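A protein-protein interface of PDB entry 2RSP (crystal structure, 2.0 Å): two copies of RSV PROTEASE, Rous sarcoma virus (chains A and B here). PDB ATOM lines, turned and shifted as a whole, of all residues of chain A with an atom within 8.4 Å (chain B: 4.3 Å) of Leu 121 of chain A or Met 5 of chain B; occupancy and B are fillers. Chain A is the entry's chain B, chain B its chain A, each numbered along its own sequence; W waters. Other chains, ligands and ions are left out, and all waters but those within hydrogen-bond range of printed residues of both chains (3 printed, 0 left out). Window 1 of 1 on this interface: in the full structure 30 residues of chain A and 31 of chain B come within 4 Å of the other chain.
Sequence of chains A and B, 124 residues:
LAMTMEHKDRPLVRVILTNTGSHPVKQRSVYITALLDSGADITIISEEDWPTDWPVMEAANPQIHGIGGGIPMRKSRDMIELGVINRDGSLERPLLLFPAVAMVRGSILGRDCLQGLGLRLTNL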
ATOM      1  N   MET A   3      10.695   6.785 -21.022  1.00  0.00           N
ATOM      2  CA  MET A   3      11.725   7.273 -21.918  1.00  0.00           C
ATOM      3  C   MET A   3      12.059   6.144 -22.877  1.00  0.00           C
ATOM      4  O   MET A   3      12.363   5.012 -22.405  1.00  0.00           O
ATOM      5  CB  MET A   3      13.085   7.618 -21.238  1.00  0.00           C
ATOM      6  CG  MET A   3      12.819   8.479 -20.011  1.00  0.00           C
ATOM      7  SD  MET A   3      14.367   9.466 -19.645  1.00  0.00           S
ATOM      8  CE  MET A   3      15.407   8.323 -20.484  1.00  0.00           C
ATOM      9  N   THR A   4      12.167   6.402 -24.138  1.00  0.00           N
ATOM     10  CA  THR A   4      12.542   5.376 -25.113  1.00  0.00           C
ATOM     11  C   THR A   4      14.037   5.217 -24.983  1.00  0.00           C
ATOM     12  O   THR A   4      14.804   6.174 -24.826  1.00  0.00           O
ATOM     13  CB  THR A   4      12.103   5.930 -26.557  1.00  0.00           C
ATOM     14  OG1 THR A   4      10.635   5.913 -26.501  1.00  0.00           O
ATOM     15  CG2 THR A   4      12.394   4.996 -27.725  1.00  0.00           C
ATOM     16  N   MET A   5      14.598   4.033 -25.195  1.00  0.00           N
ATOM     17  CA  MET A   5      16.015   3.806 -25.123  1.00  0.00           C
ATOM     18  C   MET A   5      16.535   4.079 -26.532  1.00  0.00           C
ATOM     19  O   MET A   5      16.017   3.461 -27.470  1.00  0.00           O
ATOM     20  CB  MET A   5      16.298   2.351 -24.742  1.00  0.00           C
ATOM     21  CG  MET A   5      15.783   1.949 -23.343  1.00  0.00           C
ATOM     22  SD  MET A   5      16.888   2.715 -22.125  1.00  0.00           S
ATOM     23  CE  MET A   5      16.063   4.251 -21.723  1.00  0.00           C
ATOM     24  N   LEU A  36      19.755   7.375 -15.692  1.00  0.00           N
ATOM     25  CA  LEU A  36      18.890   6.253 -15.268  1.00  0.00           C
ATOM     26  C   LEU A  36      19.662   5.060 -15.729  1.00  0.00           C
ATOM     27  O   LEU A  36      19.810   4.853 -16.936  1.00  0.00           O
ATOM     28  CB  LEU A  36      17.553   6.325 -15.928  1.00  0.00           C
ATOM     29  CG  LEU A  36      16.699   7.498 -15.580  1.00  0.00           C
ATOM     30  CD1 LEU A  36      15.430   7.553 -16.427  1.00  0.00           C
ATOM     31  CD2 LEU A  36      16.387   7.533 -14.101  1.00  0.00           C
ATOM     32  N   ASP A  37      20.289   4.373 -14.820  1.00  0.00           N
ATOM     33  CA  ASP A  37      21.195   3.246 -15.159  1.00  0.00           C
ATOM     34  C   ASP A  37      20.823   1.931 -14.503  1.00  0.00           C
ATOM     35  O   ASP A  37      21.132   1.622 -13.330  1.00  0.00           O
ATOM     36  CB  ASP A  37      22.532   3.762 -14.685  1.00  0.00           C
ATOM     37  CG  ASP A  37      23.625   2.783 -15.146  1.00  0.00           C
ATOM     38  OD1 ASP A  37      23.473   1.693 -15.672  1.00  0.00           O
ATOM     39  OD2 ASP A  37      24.708   3.297 -14.894  1.00  0.00           O
ATOM     40  N   SER A  38      20.100   1.141 -15.281  1.00  0.00           N
ATOM     41  CA  SER A  38      19.623  -0.214 -14.871  1.00  0.00           C
ATOM     42  C   SER A  38      20.795  -1.143 -14.617  1.00  0.00           C
ATOM     43  O   SER A  38      20.563  -2.222 -14.011  1.00  0.00           O
ATOM     44  CB  SER A  38      18.630  -0.682 -15.976  1.00  0.00           C
ATOM     45  OG  SER A  38      19.357  -1.149 -17.106  1.00  0.00           O
ATOM     46  N   GLY A  39      21.984  -0.745 -14.995  1.00  0.00           N
ATOM     47  CA  GLY A  39      23.252  -1.464 -14.836  1.00  0.00           C
ATOM     48  C   GLY A  39      23.792  -1.166 -13.415  1.00  0.00           C
ATOM     49  O   GLY A  39      24.596  -1.989 -12.955  1.00  0.00           O
ATOM     50  N   ALA A  40      23.304  -0.171 -12.671  1.00  0.00           N
ATOM     51  CA  ALA A  40      23.912   0.095 -11.300  1.00  0.00           C
ATOM     52  C   ALA A  40      23.017  -0.363 -10.207  1.00  0.00           C
ATOM     53  O   ALA A  40      21.764  -0.139 -10.223  1.00  0.00           O
ATOM     54  CB  ALA A  40      24.289   1.592 -11.344  1.00  0.00           C
ATOM     55  N   GLY A 110      20.802   4.339  -9.651  1.00  0.00           N
ATOM     56  CA  GLY A 110      20.813   2.917  -9.923  1.00  0.00           C
ATOM     57  C   GLY A 110      19.438   2.344  -9.635  1.00  0.00           C
ATOM     58  O   GLY A 110      18.445   3.013  -9.436  1.00  0.00           O
ATOM     59  N   ARG A 111      19.402   1.010  -9.563  1.00  0.00           N
ATOM     60  CA  ARG A 111      18.202   0.228  -9.343  1.00  0.00           C
ATOM     61  C   ARG A 111      17.478   0.457  -8.016  1.00  0.00           C
ATOM     62  O   ARG A 111      16.292   0.193  -7.982  1.00  0.00           O
ATOM     63  CB  ARG A 111      18.419  -1.239  -9.591  1.00  0.00           C
ATOM     64  CG  ARG A 111      18.753  -1.447 -11.085  1.00  0.00           C
ATOM     65  CD  ARG A 111      18.541  -2.868 -11.494  1.00  0.00           C
ATOM     66  NE  ARG A 111      19.125  -3.785 -10.515  1.00  0.00           N
ATOM     67  CZ  ARG A 111      20.432  -4.020 -10.491  1.00  0.00           C
ATOM     68  NH1 ARG A 111      20.983  -4.748  -9.439  1.00  0.00           N
ATOM     69  NH2 ARG A 111      21.334  -3.631 -11.363  1.00  0.00           N
ATOM     70  N   ASP A 112      18.190   0.939  -7.037  1.00  0.00           N
ATOM     71  CA  ASP A 112      17.533   1.270  -5.715  1.00  0.00           C
ATOM     72  C   ASP A 112      16.561   2.388  -6.109  1.00  0.00           C
ATOM     73  O   ASP A 112      15.411   2.453  -5.668  1.00  0.00           O
ATOM     74  CB  ASP A 112      18.634   1.663  -4.683  1.00  0.00           C
ATOM     75  CG  ASP A 112      19.574   2.760  -5.191  1.00  0.00           C
ATOM     76  OD1 ASP A 112      19.589   3.211  -6.392  1.00  0.00           O
ATOM     77  OD2 ASP A 112      20.412   3.283  -4.426  1.00  0.00           O
ATOM     78  N   CYS A 113      16.883   3.425  -6.866  1.00  0.00           N
ATOM     79  CA  CYS A 113      15.902   4.431  -7.284  1.00  0.00           C
ATOM     80  C   CYS A 113      14.976   3.905  -8.425  1.00  0.00           C
ATOM     81  O   CYS A 113      13.797   4.347  -8.430  1.00  0.00           O
ATOM     82  CB  CYS A 113      16.635   5.720  -7.788  1.00  0.00           C
ATOM     83  SG  CYS A 113      17.356   6.633  -6.401  1.00  0.00           S
ATOM     84  N   LEU A 114      15.457   3.132  -9.380  1.00  0.00           N
ATOM     85  CA  LEU A 114      14.559   2.660 -10.489  1.00  0.00           C
ATOM     86  C   LEU A 114      13.406   1.834  -9.902  1.00  0.00           C
ATOM     87  O   LEU A 114      12.213   2.006 -10.261  1.00  0.00           O
ATOM     88  CB  LEU A 114      15.392   1.955 -11.529  1.00  0.00           C
ATOM     89  CG  LEU A 114      16.631   2.591 -12.159  1.00  0.00           C
ATOM     90  CD1 LEU A 114      16.869   1.914 -13.517  1.00  0.00           C
ATOM     91  CD2 LEU A 114      16.421   4.109 -12.407  1.00  0.00           C
ATOM     92  N   GLN A 115      13.717   1.001  -8.854  1.00  0.00           N
ATOM     93  CA  GLN A 115      12.643   0.278  -8.238  1.00  0.00           C
ATOM     94  C   GLN A 115      11.781   1.234  -7.411  1.00  0.00           C
ATOM     95  O   GLN A 115      10.588   0.985  -7.495  1.00  0.00           O
ATOM     96  CB  GLN A 115      13.243  -0.798  -7.377  1.00  0.00           C
ATOM     97  CG  GLN A 115      12.195  -1.715  -6.800  1.00  0.00           C
ATOM     98  CD  GLN A 115      12.819  -2.733  -5.867  1.00  0.00           C
ATOM     99  OE1 GLN A 115      13.939  -3.186  -5.821  1.00  0.00           O
ATOM    100  NE2 GLN A 115      11.845  -2.983  -5.019  1.00  0.00           N
ATOM    101  N   GLY A 116      12.295   2.216  -6.673  1.00  0.00           N
ATOM    102  CA  GLY A 116      11.413   3.115  -5.954  1.00  0.00           C
ATOM    103  C   GLY A 116      10.463   3.780  -6.919  1.00  0.00           C
ATOM    104  O   GLY A 116       9.366   4.218  -6.513  1.00  0.00           O
ATOM    105  N   LEU A 117      10.916   4.002  -8.107  1.00  0.00           N
ATOM    106  CA  LEU A 117      10.077   4.693  -9.138  1.00  0.00           C
ATOM    107  C   LEU A 117       9.103   3.697  -9.836  1.00  0.00           C
ATOM    108  O   LEU A 117       8.204   4.172 -10.555  1.00  0.00           O
ATOM    109  CB  LEU A 117      10.890   5.440 -10.192  1.00  0.00           C
ATOM    110  CG  LEU A 117      11.664   6.661  -9.741  1.00  0.00           C
ATOM    111  CD1 LEU A 117      12.641   7.119 -10.790  1.00  0.00           C
ATOM    112  CD2 LEU A 117      10.731   7.852  -9.385  1.00  0.00           C
ATOM    113  N   GLY A 118       9.305   2.439  -9.635  1.00  0.00           N
ATOM    114  CA  GLY A 118       8.315   1.518 -10.238  1.00  0.00           C
ATOM    115  C   GLY A 118       8.620   1.319 -11.716  1.00  0.00           C
ATOM    116  O   GLY A 118       7.684   0.918 -12.396  1.00  0.00           O
ATOM    117  N   LEU A 119       9.818   1.510 -12.192  1.00  0.00           N
ATOM    118  CA  LEU A 119      10.084   1.322 -13.606  1.00  0.00           C
ATOM    119  C   LEU A 119      10.260  -0.086 -14.070  1.00  0.00           C
ATOM    120  O   LEU A 119      10.729  -1.046 -13.449  1.00  0.00           O
ATOM    121  CB  LEU A 119      11.316   2.159 -13.955  1.00  0.00           C
ATOM    122  CG  LEU A 119      11.339   3.638 -13.644  1.00  0.00           C
ATOM    123  CD1 LEU A 119      12.753   4.222 -13.866  1.00  0.00           C
ATOM    124  CD2 LEU A 119      10.406   4.351 -14.571  1.00  0.00           C
ATOM    125  N   ARG A 120       9.982  -0.258 -15.357  1.00  0.00           N
ATOM    126  CA  ARG A 120      10.268  -1.586 -16.038  1.00  0.00           C
ATOM    127  C   ARG A 120      10.885  -1.368 -17.409  1.00  0.00           C
ATOM    128  O   ARG A 120      10.670  -0.207 -17.914  1.00  0.00           O
ATOM    129  CB  ARG A 120       8.905  -2.244 -16.079  1.00  0.00           C
ATOM    130  CG  ARG A 120       7.925  -1.641 -17.091  1.00  0.00           C
ATOM    131  CD  ARG A 120       6.630  -2.424 -16.797  1.00  0.00           C
ATOM    132  NE  ARG A 120       5.699  -2.102 -17.878  1.00  0.00           N
ATOM    133  CZ  ARG A 120       4.926  -1.024 -17.700  1.00  0.00           C
ATOM    134  NH1 ARG A 120       5.002  -0.299 -16.578  1.00  0.00           N
ATOM    135  NH2 ARG A 120       4.046  -0.684 -18.638  1.00  0.00           N
ATOM    136  N   LEU A 121      11.636  -2.219 -18.073  1.00  0.00           N
ATOM    137  CA  LEU A 121      12.167  -2.087 -19.373  1.00  0.00           C
ATOM    138  C   LEU A 121      11.187  -2.910 -20.210  1.00  0.00           C
ATOM    139  O   LEU A 121      11.038  -4.055 -19.704  1.00  0.00           O
ATOM    140  CB  LEU A 121      13.563  -2.660 -19.687  1.00  0.00           C
ATOM    141  CG  LEU A 121      14.636  -1.729 -19.230  1.00  0.00           C
ATOM    142  CD1 LEU A 121      15.940  -2.504 -19.223  1.00  0.00           C
ATOM    143  CD2 LEU A 121      14.627  -0.618 -20.346  1.00  0.00           C
ATOM    144  N   THR A 122      10.582  -2.350 -21.240  1.00  0.00           N
ATOM    145  CA  THR A 122       9.567  -3.239 -21.926  1.00  0.00           C
ATOM    146  C   THR A 122       9.390  -2.770 -23.369  1.00  0.00           C
ATOM    147  O   THR A 122       9.649  -1.546 -23.628  1.00  0.00           O
ATOM    148  CB  THR A 122       8.235  -3.005 -21.067  1.00  0.00           C
ATOM    149  OG1 THR A 122       7.233  -3.753 -21.771  1.00  0.00           O
ATOM    150  CG2 THR A 122       7.731  -1.552 -21.079  1.00  0.00           C
ATOM    151  N   ASN A 123       8.960  -3.629 -24.282  1.00  0.00           N
ATOM    152  CA  ASN A 123       8.627  -3.388 -25.676  1.00  0.00           C
ATOM    153  C   ASN A 123       7.156  -3.769 -25.847  1.00  0.00           C
ATOM    154  O   ASN A 123       6.700  -3.914 -26.982  1.00  0.00           O
ATOM    155  CB  ASN A 123       9.567  -3.976 -26.742  1.00  0.00           C
ATOM    156  CG  ASN A 123       9.849  -5.463 -26.583  1.00  0.00           C
ATOM    157  OD1 ASN A 123       9.087  -6.115 -25.896  1.00  0.00           O
ATOM    158  ND2 ASN A 123      10.866  -5.977 -27.244  1.00  0.00           N
ATOM    159  N   LEU A 124       6.371  -3.894 -24.786  1.00  0.00           N
ATOM    160  CA  LEU A 124       4.988  -4.264 -24.697  1.00  0.00           C
ATOM    161  C   LEU A 124       4.167  -3.100 -24.262  1.00  0.00           C
ATOM    162  O   LEU A 124       4.659  -1.950 -24.163  1.00  0.00           O
ATOM    163  CB  LEU A 124       4.714  -5.489 -23.741  1.00  0.00           C
ATOM    164  CG  LEU A 124       5.668  -6.659 -23.883  1.00  0.00           C
ATOM    165  CD1 LEU A 124       5.342  -7.769 -22.850  1.00  0.00           C
ATOM    166  CD2 LEU A 124       5.417  -7.195 -25.289  1.00  0.00           C
ATOM    167  OXT LEU A 124       2.987  -3.257 -24.053  1.00  0.00           O
ATOM    168  N   LEU B   1       9.660  -8.646 -24.562  1.00  0.00           N
ATOM    169  CA  LEU B   1      10.500  -8.508 -23.306  1.00  0.00           C
ATOM    170  C   LEU B   1       9.913  -7.490 -22.330  1.00  0.00           C
ATOM    171  O   LEU B   1       9.716  -6.351 -22.827  1.00  0.00           O
ATOM    172  CB  LEU B   1      11.933  -8.113 -23.718  1.00  0.00           C
ATOM    173  CG  LEU B   1      13.063  -7.986 -22.676  1.00  0.00           C
ATOM    174  CD1 LEU B   1      13.537  -9.339 -22.158  1.00  0.00           C
ATOM    175  CD2 LEU B   1      14.364  -7.656 -23.433  1.00  0.00           C
ATOM    176  N   ALA B   2       9.660  -7.871 -21.047  1.00  0.00           N
ATOM    177  CA  ALA B   2       9.163  -6.836 -20.118  1.00  0.00           C
ATOM    178  C   ALA B   2       9.914  -7.242 -18.857  1.00  0.00           C
ATOM    179  O   ALA B   2       9.833  -8.414 -18.507  1.00  0.00           O
ATOM    180  CB  ALA B   2       7.680  -6.816 -19.949  1.00  0.00           C
ATOM    181  N   MET B   3      10.667  -6.392 -18.196  1.00  0.00           N
ATOM    182  CA  MET B   3      11.427  -6.730 -16.982  1.00  0.00           C
ATOM    183  C   MET B   3      11.315  -5.544 -16.017  1.00  0.00           C
ATOM    184  O   MET B   3      11.711  -4.391 -16.375  1.00  0.00           O
ATOM    185  CB  MET B   3      12.903  -6.891 -17.360  1.00  0.00           C
ATOM    186  CG  MET B   3      13.573  -7.564 -16.174  1.00  0.00           C
ATOM    187  SD  MET B   3      14.914  -8.687 -16.710  1.00  0.00           S
ATOM    188  CE  MET B   3      14.311  -8.969 -18.420  1.00  0.00           C
ATOM    189  N   THR B   4      10.845  -5.890 -14.824  1.00  0.00           N
ATOM    190  CA  THR B   4      10.704  -4.949 -13.696  1.00  0.00           C
ATOM    191  C   THR B   4      12.070  -4.613 -13.109  1.00  0.00           C
ATOM    192  O   THR B   4      12.895  -5.536 -13.041  1.00  0.00           O
ATOM    193  CB  THR B   4       9.711  -5.548 -12.636  1.00  0.00           C
ATOM    194  OG1 THR B   4       8.414  -5.521 -13.412  1.00  0.00           O
ATOM    195  CG2 THR B   4       9.453  -4.668 -11.407  1.00  0.00           C
ATOM    196  N   MET B   5      12.331  -3.346 -12.739  1.00  0.00           N
ATOM    197  CA  MET B   5      13.644  -3.000 -12.186  1.00  0.00           C
ATOM    198  C   MET B   5      13.541  -3.338 -10.664  1.00  0.00           C
ATOM    199  O   MET B   5      12.615  -2.845 -10.001  1.00  0.00           O
ATOM    200  CB  MET B   5      14.069  -1.537 -12.394  1.00  0.00           C
ATOM    201  CG  MET B   5      14.125  -1.188 -13.891  1.00  0.00           C
ATOM    202  SD  MET B   5      15.578  -1.920 -14.595  1.00  0.00           S
ATOM    203  CE  MET B   5      14.932  -3.360 -15.449  1.00  0.00           C
ATOM    204  N   GLU B   6      14.478  -4.136 -10.242  1.00  0.00           N
ATOM    205  CA  GLU B   6      14.464  -4.468  -8.783  1.00  0.00           C
ATOM    206  C   GLU B   6      15.838  -4.189  -8.244  1.00  0.00           C
ATOM    207  O   GLU B   6      16.847  -4.503  -8.935  1.00  0.00           O
ATOM    208  CB  GLU B   6      14.324  -6.002  -8.627  1.00  0.00           C
ATOM    209  CG  GLU B   6      12.777  -6.020  -8.729  1.00  0.00           C
ATOM    210  CD  GLU B   6      12.224  -7.412  -8.799  1.00  0.00           C
ATOM    211  OE1 GLU B   6      11.060  -7.509  -8.369  1.00  0.00           O
ATOM    212  OE2 GLU B   6      13.013  -8.294  -9.243  1.00  0.00           O
ATOM    213  N   PRO B  11      18.806  -7.186 -13.813  1.00  0.00           N
ATOM    214  CA  PRO B  11      17.902  -7.531 -14.937  1.00  0.00           C
ATOM    215  C   PRO B  11      18.674  -8.387 -15.945  1.00  0.00           C
ATOM    216  O   PRO B  11      19.176  -7.834 -16.961  1.00  0.00           O
ATOM    217  CB  PRO B  11      17.593  -6.140 -15.552  1.00  0.00           C
ATOM    218  CG  PRO B  11      18.705  -5.238 -15.140  1.00  0.00           C
ATOM    219  CD  PRO B  11      19.287  -5.813 -13.815  1.00  0.00           C
ATOM    220  N   LEU B  36      20.699  -5.975 -18.921  1.00  0.00           N
ATOM    221  CA  LEU B  36      20.028  -4.938 -19.729  1.00  0.00           C
ATOM    222  C   LEU B  36      20.571  -3.634 -19.119  1.00  0.00           C
ATOM    223  O   LEU B  36      20.098  -3.384 -17.986  1.00  0.00           O
ATOM    224  CB  LEU B  36      18.519  -5.188 -19.662  1.00  0.00           C
ATOM    225  CG  LEU B  36      17.994  -6.533 -20.242  1.00  0.00           C
ATOM    226  CD1 LEU B  36      16.499  -6.557 -20.025  1.00  0.00           C
ATOM    227  CD2 LEU B  36      18.162  -6.607 -21.777  1.00  0.00           C
ATOM    228  N   ARG B 120      11.587   0.716 -23.938  1.00  0.00           N
ATOM    229  CA  ARG B 120      11.289   1.986 -23.322  1.00  0.00           C
ATOM    230  C   ARG B 120      11.416   1.665 -21.816  1.00  0.00           C
ATOM    231  O   ARG B 120      11.105   0.535 -21.301  1.00  0.00           O
ATOM    232  CB  ARG B 120       9.953   2.697 -23.574  1.00  0.00           C
ATOM    233  CG  ARG B 120       8.715   1.986 -22.986  1.00  0.00           C
ATOM    234  CD  ARG B 120       7.500   2.613 -23.658  1.00  0.00           C
ATOM    235  NE  ARG B 120       6.299   1.994 -23.125  1.00  0.00           N
ATOM    236  CZ  ARG B 120       5.869   0.770 -23.407  1.00  0.00           C
ATOM    237  NH1 ARG B 120       6.481  -0.015 -24.293  1.00  0.00           N
ATOM    238  NH2 ARG B 120       4.823   0.382 -22.662  1.00  0.00           N
ATOM    239  N   LEU B 121      11.841   2.665 -21.091  1.00  0.00           N
ATOM    240  CA  LEU B 121      11.949   2.642 -19.614  1.00  0.00           C
ATOM    241  C   LEU B 121      10.665   3.349 -19.136  1.00  0.00           C
ATOM    242  O   LEU B 121      10.383   4.473 -19.552  1.00  0.00           O
ATOM    243  CB  LEU B 121      13.307   3.185 -19.219  1.00  0.00           C
ATOM    244  CG  LEU B 121      13.798   3.148 -17.791  1.00  0.00           C
ATOM    245  CD1 LEU B 121      13.805   1.724 -17.208  1.00  0.00           C
ATOM    246  CD2 LEU B 121      15.258   3.567 -17.851  1.00  0.00           C
HETATM  247  O   HOH W   1      10.529  -1.619 -10.385  1.00  0.00           O
HETATM  248  O   HOH W   2       8.684   0.507 -26.273  1.00  0.00           O
HETATM  249  O   HOH W   3       2.913  -1.820 -21.322  1.00  0.00           O
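Along chain B the printed residues that touch a printed residue of chain A span positions 1 to 121.
Of the 23 printed residues of chain A, 12 touch a printed residue of chain B.
Among the printed residues, no Asp or Glu carboxylate lies within 4 Å of a Lys or Arg side-chain nitrogen of the other chain.
The backbone NH of Leu 1 of chain B is in hydrogen-bond range of the side-chain amide oxygen of Asn 123 of chain A, at 2.9 Å.
The backbone carbonyl oxygen (O) of Met 3 of chain B lies within hydrogen-bond range of the backbone NH (N) of Leu 121 of chain A, 2.8 Å away.
N of Met 5 of chain B lies within hydrogen-bond range of O of Leu 119 of chain A (2.9 Å).
The guanidinium group (NE) of Arg 111 of chain A lies within hydrogen-bond range of the backbone carbonyl oxygen (O) of Glu 6 of chain B, 2.9 Å away.
O of Leu 36 of chain B sits at hydrogen-bond distance from OG of Ser 38 of chain A.
The backbone carbonyl oxygen (O) of Arg 120 of chain B sits at hydrogen-bond distance from the backbone NH (N) of Thr 122 of chain A, 2.9 Å away.
The guanidinium group (NH1) of Arg 120 of chain B lies within salt-bridge range of the chain-end carboxylate (O) of Leu 124 of chain A.
The backbone carbonyl oxygen (O) of Met 3 of chain A lies within hydrogen-bond range of the backbone NH (N) of Leu 121 of chain B, 2.7 Å away.
O of Arg 120 of chain A sits close to O of Arg 120 of chain B (3.5 Å).
Met 5 of chain A touches Leu 121 of chain B, and with the chains exchanged Leu 121 of chain A touches Met 5 of chain B.
Arg 120 of chain B touches its own counterpart, Arg 120 of chain A.
Arg 120 of chain A touches Leu 121 of chain B, and with the chains exchanged Leu 121 of chain A touches Arg 120 of chain B.
Leu 121 of chain A touches Leu 36 of chain B, but with the chains exchanged Leu 36 of chain A does not touch Leu 121 of chain B (4.1 Å).
6 positions are printed for both chains.
Of the 27 pairs that touch across the chains among the printed residues, 9 have their exchanged pair printed and touching as well.
The backbone carbonyl oxygen (O) of Pro 11 of chain B is in hydrogen-bond range of the backbone NH (N) of Leu 36 of chain B, at 3.1 Å.
The backbone carbonyl oxygen (O) of Ser 38 of chain A sits at hydrogen-bond distance from the guanidinium group (NH2) of Arg 111 of chain A, at 3.1 Å.
The backbone carbonyl oxygen (O) of Ala 40 of chain A is in hydrogen-bond range of the backbone NH (N) of Arg 111 of chain A (2.7 Å).
N of Leu 119 of chain A sits at hydrogen-bond distance from O of Leu 114 of chain A (3.1 Å).
The backbone NH (N) of Leu 124 of chain A lies within hydrogen-bond range of the side-chain hydroxyl (OG1) of Thr 122 of chain A.
Water W1 bridges the backbone carbonyl oxygen (O) of Met 5 of chain B (2.4 Å) and the backbone carbonyl oxygen (O) of Leu 119 of chain A (3.1 Å).
Water W2 lies within hydrogen-bond range of the guanidinium group of Arg 120 of chain B (3.0 Å) and the backbone carbonyl oxygen of Thr 122 of chain A (3.5 Å).
Water W3 lies within hydrogen-bond range of OXT of Leu 124 of chain A, NH2 of Arg 120 of chain A and NH2 of Arg 120 of chain B.
Of the printed residues of chain B, Leu 121 of chain A touches Ala 2, Met 3, Met 5, Leu 36 and Arg 120.
Of the printed residues of chain A, Met 5 of chain B touches Ser 38, Leu 114, Gln 115, Leu 119 and Leu 121.
Of the printed residues of chain B, Asn 123 of chain A touches Leu 1 (2.9 Å).
Of the printed residues of chain B, Leu 124 of chain A touches Ala 2 (3.8 Å) and Arg 120 (2.7 Å).
Of the printed residues of chain A, Met 3 of chain B touches Arg 120 and Leu 121.
Of the printed residues of chain A, Thr 4 of chain B touches Leu 119 (3.8 Å).
Of the printed residues of chain B, Ser 38 of chain A touches Met 5 (3.6 Å), Pro 11 (3.7 Å) and Leu 36 (2.5 Å).
The nearest printed residue of chain A that does not touch Met 5 of chain B is Arg 120 of chain A (4.3 Å).
The nearest printed residue of chain A that does not touch Pro 11 of chain B is Leu 121 of chain A (5.4 Å).
Met 3 of chain A touches Arg 120 of chain B (O to CA, 3.3 Å).
Met 5 of chain A touches Leu 121 of chain B (CE to CB, 3.9 Å).
Ser 38 of chain A touches Pro 11 of chain B.
Leu 114 of chain A touches Met 5 of chain B (CB to CB, 3.8 Å).
Gln 115 of chain A touches Met 5 of chain B (CB to O, 3.4 Å).
C of Glu 6 of chain B touches OE1 of Gln 115 of chain A, at 3.2 Å.
Arg 120 of chain A touches Met 3 of chain B.
Leu 121 of chain A touches Ala 2 of chain B (O to CA, 3.4 Å).
CD1 of Leu 121 of chain A touches CB of Leu 36 of chain B, at 3.7 Å.
Ala 2 of chain B touches Leu 124 of chain A (CB to CD1, 3.8 Å).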
